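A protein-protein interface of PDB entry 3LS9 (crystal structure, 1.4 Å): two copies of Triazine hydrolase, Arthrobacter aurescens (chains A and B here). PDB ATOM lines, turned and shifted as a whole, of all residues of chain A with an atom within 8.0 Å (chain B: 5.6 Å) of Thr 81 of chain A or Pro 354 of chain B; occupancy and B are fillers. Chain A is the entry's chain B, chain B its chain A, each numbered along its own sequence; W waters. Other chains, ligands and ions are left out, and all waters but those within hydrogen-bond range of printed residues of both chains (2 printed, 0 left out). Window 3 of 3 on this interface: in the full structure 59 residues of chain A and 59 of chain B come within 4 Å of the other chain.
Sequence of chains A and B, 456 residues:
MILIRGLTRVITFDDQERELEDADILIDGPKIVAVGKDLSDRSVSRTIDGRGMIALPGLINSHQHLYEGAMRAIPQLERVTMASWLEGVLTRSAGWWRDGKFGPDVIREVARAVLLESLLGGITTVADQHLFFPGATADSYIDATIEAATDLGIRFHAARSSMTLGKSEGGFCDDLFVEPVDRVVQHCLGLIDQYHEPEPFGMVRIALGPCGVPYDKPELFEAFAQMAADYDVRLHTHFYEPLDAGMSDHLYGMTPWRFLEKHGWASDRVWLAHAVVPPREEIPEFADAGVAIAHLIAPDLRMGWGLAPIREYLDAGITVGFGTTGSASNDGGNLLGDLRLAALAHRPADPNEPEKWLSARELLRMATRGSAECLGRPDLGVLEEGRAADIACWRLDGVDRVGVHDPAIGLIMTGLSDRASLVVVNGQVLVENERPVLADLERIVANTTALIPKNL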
ATOM      1  N   GLN A  76      38.266  10.017  19.698  1.00  0.00           N
ATOM      2  CA  GLN A  76      36.907  10.340  20.113  1.00  0.00           C
ATOM      3  C   GLN A  76      35.833   9.809  19.169  1.00  0.00           C
ATOM      4  O   GLN A  76      34.648   9.808  19.510  1.00  0.00           O
ATOM      5  CB  GLN A  76      36.762  11.855  20.264  1.00  0.00           C
ATOM      6  CG  GLN A  76      37.607  12.460  21.384  1.00  0.00           C
ATOM      7  CD  GLN A  76      39.072  12.711  21.011  1.00  0.00           C
ATOM      8  OE1 GLN A  76      39.508  12.497  19.872  1.00  0.00           O
ATOM      9  NE2 GLN A  76      39.841  13.182  21.990  1.00  0.00           N
ATOM     10  N   LEU A  77      36.232   9.369  17.978  1.00  0.00           N
ATOM     11  CA  LEU A  77      35.274   8.856  17.005  1.00  0.00           C
ATOM     12  C   LEU A  77      35.448   7.363  16.772  1.00  0.00           C
ATOM     13  O   LEU A  77      34.839   6.812  15.863  1.00  0.00           O
ATOM     14  CB  LEU A  77      35.417   9.583  15.664  1.00  0.00           C
ATOM     15  CG  LEU A  77      35.035  11.065  15.655  1.00  0.00           C
ATOM     16  CD1 LEU A  77      35.321  11.673  14.302  1.00  0.00           C
ATOM     17  CD2 LEU A  77      33.568  11.216  16.004  1.00  0.00           C
ATOM     18  N   GLU A  78      36.284   6.716  17.574  1.00  0.00           N
ATOM     19  CA  GLU A  78      36.544   5.288  17.363  1.00  0.00           C
ATOM     20  C   GLU A  78      35.318   4.415  17.603  1.00  0.00           C
ATOM     21  O   GLU A  78      35.000   3.548  16.789  1.00  0.00           O
ATOM     22  CB  GLU A  78      37.694   4.782  18.237  1.00  0.00           C
ATOM     23  CG  GLU A  78      38.108   3.357  17.837  1.00  0.00           C
ATOM     24  CD  GLU A  78      39.072   2.667  18.786  1.00  0.00           C
ATOM     25  OE1 GLU A  78      39.623   3.293  19.712  1.00  0.00           O
ATOM     26  OE2 GLU A  78      39.275   1.454  18.583  1.00  0.00           O
ATOM     27  N   ARG A  79      34.646   4.632  18.728  1.00  0.00           N
ATOM     28  CA  ARG A  79      33.487   3.834  19.106  1.00  0.00           C
ATOM     29  C   ARG A  79      32.316   4.761  19.400  1.00  0.00           C
ATOM     30  O   ARG A  79      32.116   5.182  20.537  1.00  0.00           O
ATOM     31  CB  ARG A  79      33.810   2.967  20.325  1.00  0.00           C
ATOM     32  CG  ARG A  79      34.891   1.901  20.080  1.00  0.00           C
ATOM     33  CD  ARG A  79      35.172   1.098  21.347  1.00  0.00           C
ATOM     34  NE  ARG A  79      35.858   1.907  22.350  1.00  0.00           N
ATOM     35  CZ  ARG A  79      36.054   1.530  23.607  1.00  0.00           C
ATOM     36  NH1 ARG A  79      35.603   0.355  24.033  1.00  0.00           N
ATOM     37  NH2 ARG A  79      36.707   2.327  24.443  1.00  0.00           N
ATOM     38  N   VAL A  80      31.542   5.046  18.362  1.00  0.00           N
ATOM     39  CA  VAL A  80      30.435   6.001  18.447  1.00  0.00           C
ATOM     40  C   VAL A  80      29.252   5.525  17.626  1.00  0.00           C
ATOM     41  O   VAL A  80      29.416   4.880  16.589  1.00  0.00           O
ATOM     42  CB  VAL A  80      30.834   7.418  17.926  1.00  0.00           C
ATOM     43  CG1 VAL A  80      31.718   8.127  18.933  1.00  0.00           C
ATOM     44  CG2 VAL A  80      31.515   7.340  16.560  1.00  0.00           C
ATOM     45  N   THR A  81      28.052   5.863  18.087  1.00  0.00           N
ATOM     46  CA  THR A  81      26.843   5.676  17.299  1.00  0.00           C
ATOM     47  C   THR A  81      26.768   6.773  16.233  1.00  0.00           C
ATOM     48  O   THR A  81      27.522   7.748  16.284  1.00  0.00           O
ATOM     49  CB  THR A  81      25.590   5.784  18.185  1.00  0.00           C
ATOM     50  OG1 THR A  81      25.533   7.097  18.752  1.00  0.00           O
ATOM     51  CG2 THR A  81      25.633   4.758  19.304  1.00  0.00           C
ATOM     52  N   MET A  82      25.866   6.616  15.268  1.00  0.00           N
ATOM     53  CA  MET A  82      25.752   7.582  14.172  1.00  0.00           C
ATOM     54  C   MET A  82      25.507   9.008  14.652  1.00  0.00           C
ATOM     55  O   MET A  82      26.115   9.945  14.143  1.00  0.00           O
ATOM     56  CB  MET A  82      24.651   7.172  13.186  1.00  0.00           C
ATOM     57  CG  MET A  82      24.532   8.107  11.982  1.00  0.00           C
ATOM     58  SD  MET A  82      26.053   8.179  11.020  1.00  0.00           S
ATOM     59  CE  MET A  82      25.444   8.926   9.513  1.00  0.00           C
ATOM     60  N   ALA A  83      24.613   9.190  15.617  1.00  0.00           N
ATOM     61  CA  ALA A  83      24.327  10.537  16.105  1.00  0.00           C
ATOM     62  C   ALA A  83      25.599  11.245  16.569  1.00  0.00           C
ATOM     63  O   ALA A  83      25.836  12.399  16.205  1.00  0.00           O
ATOM     64  CB  ALA A  83      23.288  10.504  17.223  1.00  0.00           C
ATOM     65  N   SER A  84      26.417  10.551  17.361  1.00  0.00           N
ATOM     66  CA  SER A  84      27.666  11.106  17.876  1.00  0.00           C
ATOM     67  C   SER A  84      28.689  11.281  16.762  1.00  0.00           C
ATOM     68  O   SER A  84      29.439  12.257  16.737  1.00  0.00           O
ATOM     69  CB  SER A  84      28.263  10.193  18.951  1.00  0.00           C
ATOM     70  OG  SER A  84      27.385  10.073  20.060  1.00  0.00           O
ATOM     71  N   TRP A  85      28.716  10.323  15.841  1.00  0.00           N
ATOM     72  CA  TRP A  85      29.640  10.373  14.716  1.00  0.00           C
ATOM     73  C   TRP A  85      29.368  11.585  13.835  1.00  0.00           C
ATOM     74  O   TRP A  85      30.278  12.344  13.524  1.00  0.00           O
ATOM     75  CB  TRP A  85      29.528   9.091  13.892  1.00  0.00           C
ATOM     76  CG  TRP A  85      30.531   8.985  12.779  1.00  0.00           C
ATOM     77  CD1 TRP A  85      31.775   8.422  12.843  1.00  0.00           C
ATOM     78  CD2 TRP A  85      30.364   9.439  11.434  1.00  0.00           C
ATOM     79  NE1 TRP A  85      32.391   8.498  11.613  1.00  0.00           N
ATOM     80  CE2 TRP A  85      31.542   9.107  10.731  1.00  0.00           C
ATOM     81  CE3 TRP A  85      29.326  10.074  10.750  1.00  0.00           C
ATOM     82  CZ2 TRP A  85      31.718   9.417   9.386  1.00  0.00           C
ATOM     83  CZ3 TRP A  85      29.503  10.376   9.412  1.00  0.00           C
ATOM     84  CH2 TRP A  85      30.688  10.042   8.745  1.00  0.00           C
ATOM     85  N   LEU A  86      28.111  11.765  13.448  1.00  0.00           N
ATOM     86  CA  LEU A  86      27.741  12.859  12.560  1.00  0.00           C
ATOM     87  C   LEU A  86      28.078  14.190  13.213  1.00  0.00           C
ATOM     88  O   LEU A  86      28.644  15.079  12.571  1.00  0.00           O
ATOM     89  CB  LEU A  86      26.253  12.783  12.205  1.00  0.00           C
ATOM     90  CG  LEU A  86      25.787  13.688  11.062  1.00  0.00           C
ATOM     91  CD1 LEU A  86      26.679  13.502   9.847  1.00  0.00           C
ATOM     92  CD2 LEU A  86      24.328  13.412  10.717  1.00  0.00           C
ATOM     93  N   GLU A  87      27.747  14.328  14.491  1.00  0.00           N
ATOM     94  CA  GLU A  87      28.058  15.556  15.215  1.00  0.00           C
ATOM     95  C   GLU A  87      29.568  15.805  15.252  1.00  0.00           C
ATOM     96  O   GLU A  87      30.027  16.923  15.025  1.00  0.00           O
ATOM     97  CB  GLU A  87      27.486  15.510  16.633  1.00  0.00           C
ATOM     98  CG  GLU A  87      27.632  16.817  17.406  1.00  0.00           C
ATOM     99  CD  GLU A  87      26.810  17.957  16.821  1.00  0.00           C
ATOM    100  OE1 GLU A  87      25.882  17.692  16.026  1.00  0.00           O
ATOM    101  OE2 GLU A  87      27.091  19.125  17.167  1.00  0.00           O
ATOM    102  N   GLY A  88      30.344  14.763  15.524  1.00  0.00           N
ATOM    103  CA  GLY A  88      31.789  14.893  15.584  1.00  0.00           C
ATOM    104  C   GLY A  88      32.405  15.275  14.252  1.00  0.00           C
ATOM    105  O   GLY A  88      33.327  16.094  14.196  1.00  0.00           O
ATOM    106  N   ARG A 302      31.042  -0.759  11.304  1.00  0.00           N
ATOM    107  CA  ARG A 302      31.655   0.253  12.151  1.00  0.00           C
ATOM    108  C   ARG A 302      30.632   1.025  12.982  1.00  0.00           C
ATOM    109  O   ARG A 302      30.893   1.378  14.133  1.00  0.00           O
ATOM    110  CB  ARG A 302      32.465   1.226  11.311  1.00  0.00           C
ATOM    111  CG  ARG A 302      33.451   2.033  12.133  1.00  0.00           C
ATOM    112  CD  ARG A 302      33.616   3.363  11.504  1.00  0.00           C
ATOM    113  NE  ARG A 302      34.790   4.104  11.954  1.00  0.00           N
ATOM    114  CZ  ARG A 302      34.812   4.931  12.994  1.00  0.00           C
ATOM    115  NH1 ARG A 302      33.736   5.090  13.764  1.00  0.00           N
ATOM    116  NH2 ARG A 302      35.933   5.581  13.278  1.00  0.00           N
ATOM    117  N   MET A 303      29.476   1.305  12.388  1.00  0.00           N
ATOM    118  CA  MET A 303      28.441   2.071  13.070  1.00  0.00           C
ATOM    119  C   MET A 303      27.537   1.193  13.925  1.00  0.00           C
ATOM    120  O   MET A 303      26.652   1.690  14.617  1.00  0.00           O
ATOM    121  CB  MET A 303      27.602   2.856  12.052  1.00  0.00           C
ATOM    122  CG  MET A 303      28.423   3.721  11.088  1.00  0.00           C
ATOM    123  SD  MET A 303      29.709   4.716  11.882  1.00  0.00           S
ATOM    124  CE  MET A 303      28.691   5.568  13.056  1.00  0.00           C
ATOM    125  N   GLY A 304      27.766  -0.115  13.891  1.00  0.00           N
ATOM    126  CA  GLY A 304      26.929  -1.048  14.618  1.00  0.00           C
ATOM    127  C   GLY A 304      25.612  -1.353  13.924  1.00  0.00           C
ATOM    128  O   GLY A 304      24.720  -1.953  14.525  1.00  0.00           O
ATOM    129  N   TRP A 305      25.496  -0.965  12.656  1.00  0.00           N
ATOM    130  CA  TRP A 305      24.241  -1.103  11.916  1.00  0.00           C
ATOM    131  C   TRP A 305      23.904  -2.544  11.541  1.00  0.00           C
ATOM    132  O   TRP A 305      22.736  -2.924  11.515  1.00  0.00           O
ATOM    133  CB  TRP A 305      24.262  -0.247  10.653  1.00  0.00           C
ATOM    134  CG  TRP A 305      24.286   1.227  10.898  1.00  0.00           C
ATOM    135  CD1 TRP A 305      24.031   1.873  12.074  1.00  0.00           C
ATOM    136  CD2 TRP A 305      24.563   2.240   9.932  1.00  0.00           C
ATOM    137  NE1 TRP A 305      24.139   3.232  11.896  1.00  0.00           N
ATOM    138  CE2 TRP A 305      24.467   3.484  10.588  1.00  0.00           C
ATOM    139  CE3 TRP A 305      24.892   2.216   8.575  1.00  0.00           C
ATOM    140  CZ2 TRP A 305      24.683   4.695   9.927  1.00  0.00           C
ATOM    141  CZ3 TRP A 305      25.106   3.416   7.920  1.00  0.00           C
ATOM    142  CH2 TRP A 305      25.003   4.639   8.595  1.00  0.00           C
ATOM    143  N   ASP B 350      25.857  -4.915  19.782  1.00  0.00           N
ATOM    144  CA  ASP B 350      25.502  -3.932  20.808  1.00  0.00           C
ATOM    145  C   ASP B 350      25.339  -2.571  20.161  1.00  0.00           C
ATOM    146  O   ASP B 350      26.123  -1.657  20.421  1.00  0.00           O
ATOM    147  CB  ASP B 350      26.587  -3.874  21.887  1.00  0.00           C
ATOM    148  CG  ASP B 350      26.634  -5.132  22.726  1.00  0.00           C
ATOM    149  OD1 ASP B 350      25.688  -5.351  23.513  1.00  0.00           O
ATOM    150  OD2 ASP B 350      27.605  -5.910  22.596  1.00  0.00           O
ATOM    151  N   PRO B 351      24.304  -2.430  19.318  1.00  0.00           N
ATOM    152  CA  PRO B 351      24.184  -1.255  18.446  1.00  0.00           C
ATOM    153  C   PRO B 351      24.112   0.060  19.210  1.00  0.00           C
ATOM    154  O   PRO B 351      24.551   1.084  18.682  1.00  0.00           O
ATOM    155  CB  PRO B 351      22.872  -1.488  17.688  1.00  0.00           C
ATOM    156  CG  PRO B 351      22.420  -2.853  18.014  1.00  0.00           C
ATOM    157  CD  PRO B 351      23.165  -3.358  19.196  1.00  0.00           C
ATOM    158  N   ASN B 352      23.573   0.038  20.426  1.00  0.00           N
ATOM    159  CA  ASN B 352      23.351   1.273  21.175  1.00  0.00           C
ATOM    160  C   ASN B 352      24.311   1.463  22.346  1.00  0.00           C
ATOM    161  O   ASN B 352      24.159   2.397  23.134  1.00  0.00           O
ATOM    162  CB  ASN B 352      21.913   1.319  21.706  1.00  0.00           C
ATOM    163  CG  ASN B 352      20.896   1.672  20.634  1.00  0.00           C
ATOM    164  OD1 ASN B 352      20.996   1.241  19.487  1.00  0.00           O
ATOM    165  ND2 ASN B 352      19.897   2.464  21.016  1.00  0.00           N
ATOM    166  N   GLU B 353      25.294   0.577  22.471  1.00  0.00           N
ATOM    167  CA  GLU B 353      26.242   0.639  23.579  1.00  0.00           C
ATOM    168  C   GLU B 353      27.685   0.520  23.095  1.00  0.00           C
ATOM    169  O   GLU B 353      28.346  -0.501  23.326  1.00  0.00           O
ATOM    170  CB  GLU B 353      25.940  -0.465  24.596  1.00  0.00           C
ATOM    171  CG  GLU B 353      24.556  -0.340  25.231  1.00  0.00           C
ATOM    172  CD  GLU B 353      24.404  -1.223  26.454  1.00  0.00           C
ATOM    173  OE1 GLU B 353      24.603  -0.720  27.579  1.00  0.00           O
ATOM    174  OE2 GLU B 353      24.092  -2.417  26.289  1.00  0.00           O
ATOM    175  N   PRO B 354      28.192   1.570  22.440  1.00  0.00           N
ATOM    176  CA  PRO B 354      29.536   1.491  21.858  1.00  0.00           C
ATOM    177  C   PRO B 354      30.641   1.303  22.897  1.00  0.00           C
ATOM    178  O   PRO B 354      31.745   0.886  22.552  1.00  0.00           O
ATOM    179  CB  PRO B 354      29.688   2.829  21.116  1.00  0.00           C
ATOM    180  CG  PRO B 354      28.656   3.742  21.750  1.00  0.00           C
ATOM    181  CD  PRO B 354      27.521   2.846  22.136  1.00  0.00           C
ATOM    182  N   GLU B 355      30.363   1.579  24.167  1.00  0.00           N
ATOM    183  CA  GLU B 355      31.363   1.342  25.201  1.00  0.00           C
ATOM    184  C   GLU B 355      31.673  -0.157  25.357  1.00  0.00           C
ATOM    185  O   GLU B 355      32.716  -0.534  25.895  1.00  0.00           O
ATOM    186  CB  GLU B 355      30.918   1.955  26.537  1.00  0.00           C
ATOM    187  CG  GLU B 355      29.714   1.280  27.188  1.00  0.00           C
ATOM    188  CD  GLU B 355      28.356   1.753  26.656  1.00  0.00           C
ATOM    189  OE1 GLU B 355      28.289   2.574  25.708  1.00  0.00           O
ATOM    190  OE2 GLU B 355      27.334   1.289  27.212  1.00  0.00           O
ATOM    191  N   LYS B 356      30.772  -1.006  24.869  1.00  0.00           N
ATOM    192  CA  LYS B 356      30.992  -2.452  24.919  1.00  0.00           C
ATOM    193  C   LYS B 356      31.885  -2.954  23.786  1.00  0.00           C
ATOM    194  O   LYS B 356      32.487  -4.013  23.898  1.00  0.00           O
ATOM    195  CB  LYS B 356      29.661  -3.208  24.908  1.00  0.00           C
ATOM    196  CG  LYS B 356      28.845  -2.992  26.179  1.00  0.00           C
ATOM    197  CD  LYS B 356      27.574  -3.824  26.199  1.00  0.00           C
ATOM    198  CE  LYS B 356      26.922  -3.779  27.580  1.00  0.00           C
ATOM    199  NZ  LYS B 356      25.543  -4.349  27.575  1.00  0.00           N
ATOM    200  N   TRP B 357      31.946  -2.209  22.688  1.00  0.00           N
ATOM    201  CA  TRP B 357      32.738  -2.608  21.526  1.00  0.00           C
ATOM    202  C   TRP B 357      34.210  -2.707  21.906  1.00  0.00           C
ATOM    203  O   TRP B 357      34.700  -1.937  22.733  1.00  0.00           O
ATOM    204  CB  TRP B 357      32.569  -1.587  20.401  1.00  0.00           C
ATOM    205  CG  TRP B 357      31.138  -1.340  20.004  1.00  0.00           C
ATOM    206  CD1 TRP B 357      30.042  -2.051  20.393  1.00  0.00           C
ATOM    207  CD2 TRP B 357      30.658  -0.312  19.124  1.00  0.00           C
ATOM    208  NE1 TRP B 357      28.910  -1.529  19.813  1.00  0.00           N
ATOM    209  CE2 TRP B 357      29.263  -0.458  19.033  1.00  0.00           C
ATOM    210  CE3 TRP B 357      31.277   0.715  18.401  1.00  0.00           C
ATOM    211  CZ2 TRP B 357      28.475   0.388  18.253  1.00  0.00           C
ATOM    212  CZ3 TRP B 357      30.492   1.551  17.632  1.00  0.00           C
ATOM    213  CH2 TRP B 357      29.109   1.379  17.561  1.00  0.00           C
HETATM  214  O   HOH W   1      34.921   1.216  26.890  1.00  0.00           O
HETATM  215  O   HOH W   2      24.443   1.587  15.938  1.00  0.00           O
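Water W2 lies within hydrogen-bond range of O of Met 303 of chain A (2.6 Å) and O of Pro 351 of chain B (2.8 Å). Water W1 bridges the backbone carbonyl oxygen (O) of Glu 355 of chain B (3.0 Å) and the guanidinium group (NH1) of Arg 79 of chain A (3.1 Å).
The backbone carbonyl oxygen of Trp 357 of chain B lies within hydrogen-bond range of the guanidinium group of Arg 79 of chain A, 2.8 Å away.
Arg 79 of chain A touches Pro 354 of chain B. NH1 of Arg 79 of chain A touches O of Glu 355 of chain B (3.5 Å). Pro 354 of chain B touches Val 80 of chain A. Trp 357 of chain B touches Val 80 of chain A. Pro 351 of chain B touches Thr 81 of chain A. Thr 81 of chain A touches Pro 354 of chain B (CG2 to CD, 3.9 Å). Arg 302 of chain A touches Trp 357 of chain B (O to CZ3, 3.5 Å). Met 303 of chain A touches Trp 357 of chain B (O to CH2, 3.8 Å). Pro 351 of chain B touches Gly 304 of chain A.
The indole nitrogen of Trp 357 of chain B lies within hydrogen-bond range of the backbone carbonyl oxygen of Asp 350 of chain B, 2.9 Å away. O of Leu 77 of chain A sits at hydrogen-bond distance from NH1 of Arg 302 of chain A, 2.9 Å away.
Of the printed residues of chain B, Thr 81 of chain A touches Pro 351 and Pro 354. Of the printed residues of chain A, Pro 354 of chain B touches Arg 79, Val 80 and Thr 81. Of the printed residues of chain B, Arg 79 of chain A touches Pro 354, Glu 355 and Trp 357. Of the printed residues of chain B, Met 303 of chain A touches Trp 357. Of the printed residues of chain B, Arg 302 of chain A touches Trp 357. Of the printed residues of chain A, Trp 357 of chain B touches Arg 79, Val 80, Arg 302 and Met 303. The nearest residue of chain B that does not touch Thr 81 of chain A is Asn 352 of chain B (4.6 Å). The nearest printed residue of chain A that does not touch Pro 354 of chain B is Ser 84 of chain A (6.7 Å).
Of the 17 printed residues of chain A, 6 touch a printed residue of chain B. Hydrophobic or aromatic side chains of chain B within 4 Å of the printed part of chain A: Pro 351, Pro 354 and Trp 357. Among the printed residues, no Asp or Glu carboxylate lies within 4 Å of a Lys or Arg side-chain nitrogen of the other chain.
No position is printed for both chains.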
